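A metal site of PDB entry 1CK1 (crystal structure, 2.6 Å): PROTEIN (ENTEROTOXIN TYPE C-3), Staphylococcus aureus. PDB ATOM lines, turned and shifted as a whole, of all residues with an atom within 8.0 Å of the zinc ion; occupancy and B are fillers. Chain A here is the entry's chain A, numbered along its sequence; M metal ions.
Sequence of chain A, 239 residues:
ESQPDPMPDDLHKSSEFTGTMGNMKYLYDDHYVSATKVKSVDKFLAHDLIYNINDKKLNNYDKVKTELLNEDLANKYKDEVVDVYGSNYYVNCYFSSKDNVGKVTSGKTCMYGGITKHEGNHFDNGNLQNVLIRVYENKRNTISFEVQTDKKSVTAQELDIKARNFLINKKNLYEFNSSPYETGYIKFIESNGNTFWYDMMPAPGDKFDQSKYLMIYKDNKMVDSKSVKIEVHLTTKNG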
ATOM      1  N   ALA A  35       9.462   3.806  -9.910  1.00  0.00           N
ATOM      2  CA  ALA A  35       8.204   3.913  -9.161  1.00  0.00           C
ATOM      3  C   ALA A  35       6.975   3.794 -10.071  1.00  0.00           C
ATOM      4  O   ALA A  35       6.962   4.267 -11.207  1.00  0.00           O
ATOM      5  CB  ALA A  35       8.164   5.224  -8.389  1.00  0.00           C
ATOM      6  N   THR A  36       5.910   3.206  -9.522  1.00  0.00           N
ATOM      7  CA  THR A  36       4.671   2.988 -10.239  1.00  0.00           C
ATOM      8  C   THR A  36       3.424   3.660  -9.636  1.00  0.00           C
ATOM      9  O   THR A  36       3.157   3.545  -8.434  1.00  0.00           O
ATOM     10  CB  THR A  36       4.447   1.459 -10.435  1.00  0.00           C
ATOM     11  OG1 THR A  36       4.913   1.077 -11.738  1.00  0.00           O
ATOM     12  CG2 THR A  36       2.985   1.046 -10.236  1.00  0.00           C
ATOM     13  N   LYS A  37       2.710   4.408 -10.487  1.00  0.00           N
ATOM     14  CA  LYS A  37       1.465   5.098 -10.127  1.00  0.00           C
ATOM     15  C   LYS A  37       1.500   5.954  -8.847  1.00  0.00           C
ATOM     16  O   LYS A  37       0.679   5.778  -7.948  1.00  0.00           O
ATOM     17  CB  LYS A  37       0.299   4.098 -10.058  1.00  0.00           C
ATOM     18  CG  LYS A  37       0.162   3.226 -11.305  1.00  0.00           C
ATOM     19  CD  LYS A  37      -0.786   2.067 -11.080  1.00  0.00           C
ATOM     20  CE  LYS A  37      -2.212   2.545 -10.850  1.00  0.00           C
ATOM     21  NZ  LYS A  37      -3.140   1.396 -10.732  1.00  0.00           N
ATOM     22  N   VAL A  38       2.405   6.921  -8.803  1.00  0.00           N
ATOM     23  CA  VAL A  38       2.543   7.792  -7.640  1.00  0.00           C
ATOM     24  C   VAL A  38       2.157   9.253  -7.928  1.00  0.00           C
ATOM     25  O   VAL A  38       2.135   9.692  -9.073  1.00  0.00           O
ATOM     26  CB  VAL A  38       3.994   7.752  -7.078  1.00  0.00           C
ATOM     27  CG1 VAL A  38       4.294   6.386  -6.489  1.00  0.00           C
ATOM     28  CG2 VAL A  38       4.994   8.102  -8.171  1.00  0.00           C
ATOM     29  N   VAL A  81      -0.935  11.437 -11.533  1.00  0.00           N
ATOM     30  CA  VAL A  81      -0.516  10.087 -11.157  1.00  0.00           C
ATOM     31  C   VAL A  81       0.504   9.766 -12.242  1.00  0.00           C
ATOM     32  O   VAL A  81       0.176   9.775 -13.431  1.00  0.00           O
ATOM     33  CB  VAL A  81      -1.694   9.077 -11.182  1.00  0.00           C
ATOM     34  CG1 VAL A  81      -1.180   7.654 -10.979  1.00  0.00           C
ATOM     35  CG2 VAL A  81      -2.699   9.429 -10.081  1.00  0.00           C
ATOM     36  N   VAL A  82       1.752   9.573 -11.830  1.00  0.00           N
ATOM     37  CA  VAL A  82       2.832   9.319 -12.775  1.00  0.00           C
ATOM     38  C   VAL A  82       3.718   8.121 -12.452  1.00  0.00           C
ATOM     39  O   VAL A  82       3.635   7.549 -11.359  1.00  0.00           O
ATOM     40  CB  VAL A  82       3.756  10.578 -12.887  1.00  0.00           C
ATOM     41  CG1 VAL A  82       2.976  11.786 -13.403  1.00  0.00           C
ATOM     42  CG2 VAL A  82       4.391  10.900 -11.539  1.00  0.00           C
ATOM     43  N   ASP A  83       4.532   7.727 -13.420  1.00  0.00           N
ATOM     44  CA  ASP A  83       5.506   6.651 -13.258  1.00  0.00           C
ATOM     45  C   ASP A  83       6.863   7.358 -13.274  1.00  0.00           C
ATOM     46  O   ASP A  83       7.048   8.349 -13.980  1.00  0.00           O
ATOM     47  CB  ASP A  83       5.445   5.652 -14.411  1.00  0.00           C
ATOM     48  CG  ASP A  83       4.152   4.889 -14.449  1.00  0.00           C
ATOM     49  OD1 ASP A  83       3.549   4.661 -13.379  1.00  0.00           O
ATOM     50  OD2 ASP A  83       3.747   4.505 -15.558  1.00  0.00           O
ATOM     51  N   VAL A  84       7.805   6.843 -12.488  1.00  0.00           N
ATOM     52  CA  VAL A  84       9.123   7.463 -12.405  1.00  0.00           C
ATOM     53  C   VAL A  84      10.270   6.512 -12.765  1.00  0.00           C
ATOM     54  O   VAL A  84      10.239   5.336 -12.420  1.00  0.00           O
ATOM     55  CB  VAL A  84       9.362   8.068 -10.990  1.00  0.00           C
ATOM     56  CG1 VAL A  84      10.571   8.985 -10.999  1.00  0.00           C
ATOM     57  CG2 VAL A  84       8.138   8.847 -10.517  1.00  0.00           C
ATOM     58  N   THR A 116       6.676  10.490 -16.362  1.00  0.00           N
ATOM     59  CA  THR A 116       5.718  10.238 -17.451  1.00  0.00           C
ATOM     60  C   THR A 116       4.328   9.991 -16.848  1.00  0.00           C
ATOM     61  O   THR A 116       4.223   9.457 -15.746  1.00  0.00           O
ATOM     62  CB  THR A 116       6.105   9.016 -18.376  1.00  0.00           C
ATOM     63  OG1 THR A 116       6.247   7.822 -17.583  1.00  0.00           O
ATOM     64  CG2 THR A 116       7.390   9.282 -19.147  1.00  0.00           C
ATOM     65  N   LYS A 117       3.273  10.417 -17.561  1.00  0.00           N
ATOM     66  CA  LYS A 117       1.893  10.222 -17.106  1.00  0.00           C
ATOM     67  C   LYS A 117       1.572   8.723 -17.193  1.00  0.00           C
ATOM     68  O   LYS A 117       1.988   8.052 -18.134  1.00  0.00           O
ATOM     69  CB  LYS A 117       0.900  10.994 -17.995  1.00  0.00           C
ATOM     70  CG  LYS A 117       1.041  12.513 -17.988  1.00  0.00           C
ATOM     71  CD  LYS A 117       0.182  13.147 -19.085  1.00  0.00           C
ATOM     72  CE  LYS A 117       0.350  14.668 -19.154  1.00  0.00           C
ATOM     73  NZ  LYS A 117      -0.403  15.287 -20.291  1.00  0.00           N
ATOM     74  N   HIS A 118       0.872   8.211 -16.179  1.00  0.00           N
ATOM     75  CA  HIS A 118       0.510   6.789 -16.110  1.00  0.00           C
ATOM     76  C   HIS A 118      -0.655   6.409 -17.027  1.00  0.00           C
ATOM     77  O   HIS A 118      -0.574   5.418 -17.762  1.00  0.00           O
ATOM     78  CB  HIS A 118       0.198   6.400 -14.651  1.00  0.00           C
ATOM     79  CG  HIS A 118      -0.529   5.092 -14.517  1.00  0.00           C
ATOM     80  ND1 HIS A 118       0.058   3.878 -14.765  1.00  0.00           N
ATOM     81  CD2 HIS A 118      -1.822   4.821 -14.201  1.00  0.00           C
ATOM     82  CE1 HIS A 118      -0.827   2.911 -14.631  1.00  0.00           C
ATOM     83  NE2 HIS A 118      -1.982   3.455 -14.281  1.00  0.00           N
ATOM     84  N   GLU A 119      -1.721   7.208 -16.979  1.00  0.00           N
ATOM     85  CA  GLU A 119      -2.923   6.972 -17.777  1.00  0.00           C
ATOM     86  C   GLU A 119      -2.716   7.072 -19.287  1.00  0.00           C
ATOM     87  O   GLU A 119      -2.225   8.093 -19.796  1.00  0.00           O
ATOM     88  CB  GLU A 119      -4.030   7.920 -17.312  1.00  0.00           C
ATOM     89  CG  GLU A 119      -5.320   7.864 -18.126  1.00  0.00           C
ATOM     90  CD  GLU A 119      -5.612   9.170 -18.836  1.00  0.00           C
ATOM     91  OE1 GLU A 119      -5.063   9.374 -19.944  1.00  0.00           O
ATOM     92  OE2 GLU A 119      -6.367   9.993 -18.292  1.00  0.00           O
ATOM     93  N   GLY A 120      -3.072   5.995 -19.975  1.00  0.00           N
ATOM     94  CA  GLY A 120      -2.951   5.918 -21.423  1.00  0.00           C
ATOM     95  C   GLY A 120      -1.559   5.837 -22.017  1.00  0.00           C
ATOM     96  O   GLY A 120      -1.389   6.101 -23.216  1.00  0.00           O
ATOM     97  N   ASN A 121      -0.584   5.415 -21.223  1.00  0.00           N
ATOM     98  CA  ASN A 121       0.802   5.324 -21.706  1.00  0.00           C
ATOM     99  C   ASN A 121       1.375   3.913 -21.851  1.00  0.00           C
ATOM    100  O   ASN A 121       2.576   3.760 -22.104  1.00  0.00           O
ATOM    101  CB  ASN A 121       1.726   6.181 -20.830  1.00  0.00           C
ATOM    102  CG  ASN A 121       2.968   6.655 -21.569  1.00  0.00           C
ATOM    103  OD1 ASN A 121       2.902   6.944 -22.771  1.00  0.00           O
ATOM    104  ND2 ASN A 121       4.083   6.741 -20.862  1.00  0.00           N
ATOM    105  N   HIS A 122       0.536   2.900 -21.708  1.00  0.00           N
ATOM    106  CA  HIS A 122       0.997   1.516 -21.831  1.00  0.00           C
ATOM    107  C   HIS A 122       0.372   0.761 -22.996  1.00  0.00           C
ATOM    108  O   HIS A 122      -0.750   1.050 -23.418  1.00  0.00           O
ATOM    109  CB  HIS A 122       0.784   0.746 -20.527  1.00  0.00           C
ATOM    110  CG  HIS A 122       1.514   1.340 -19.365  1.00  0.00           C
ATOM    111  ND1 HIS A 122       2.894   1.393 -19.310  1.00  0.00           N
ATOM    112  CD2 HIS A 122       1.066   1.949 -18.251  1.00  0.00           C
ATOM    113  CE1 HIS A 122       3.255   2.015 -18.208  1.00  0.00           C
ATOM    114  NE2 HIS A 122       2.171   2.366 -17.543  1.00  0.00           N
ATOM    115  N   ASP A 150       7.854  -0.410 -21.236  1.00  0.00           N
ATOM    116  CA  ASP A 150       6.410  -0.606 -21.161  1.00  0.00           C
ATOM    117  C   ASP A 150       5.642   0.695 -21.472  1.00  0.00           C
ATOM    118  O   ASP A 150       4.412   0.736 -21.406  1.00  0.00           O
ATOM    119  CB  ASP A 150       6.029  -1.127 -19.758  1.00  0.00           C
ATOM    120  CG  ASP A 150       6.360  -0.140 -18.622  1.00  0.00           C
ATOM    121  OD1 ASP A 150       7.390   0.566 -18.678  1.00  0.00           O
ATOM    122  OD2 ASP A 150       5.579  -0.104 -17.646  1.00  0.00           O
ATOM    123  N   LYS A 151       6.387   1.747 -21.838  1.00  0.00           N
ATOM    124  CA  LYS A 151       5.809   3.055 -22.118  1.00  0.00           C
ATOM    125  C   LYS A 151       5.788   3.466 -23.600  1.00  0.00           C
ATOM    126  O   LYS A 151       6.744   3.198 -24.339  1.00  0.00           O
ATOM    127  CB  LYS A 151       6.569   4.126 -21.317  1.00  0.00           C
ATOM    128  CG  LYS A 151       6.677   3.831 -19.819  1.00  0.00           C
ATOM    129  CD  LYS A 151       7.586   4.840 -19.116  1.00  0.00           C
ATOM    130  CE  LYS A 151       7.826   4.478 -17.649  1.00  0.00           C
ATOM    131  NZ  LYS A 151       8.570   3.205 -17.486  1.00  0.00           N
HETATM  132 ZN    ZN M   1       2.040   3.166 -15.474  1.00  0.00          ZN
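The side-chain carboxylate of Asp 83 lies within hydrogen-bond range of the backbone NH of Lys 37 (3.0 Å). The backbone NH (N) of Asp 83 sits at hydrogen-bond distance from the backbone carbonyl oxygen (O) of Thr 116 (2.9 Å). N of His 118 lies within hydrogen-bond range of O of Val 81 (3.2 Å). The backbone carbonyl oxygen (O) of Asp 150 sits at hydrogen-bond distance from a ring nitrogen (ND1) of His 122 (2.7 Å).
Of the 17 residues printed, 3 come within 4 Å of the zinc ion.
The zinc ion is bound by the side-chain carboxylate (OD2) of Asp 83, a ring nitrogen (ND1) of His 118 and a ring nitrogen (NE2) of His 122. The zinc ion has three donor atoms within binding distance.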
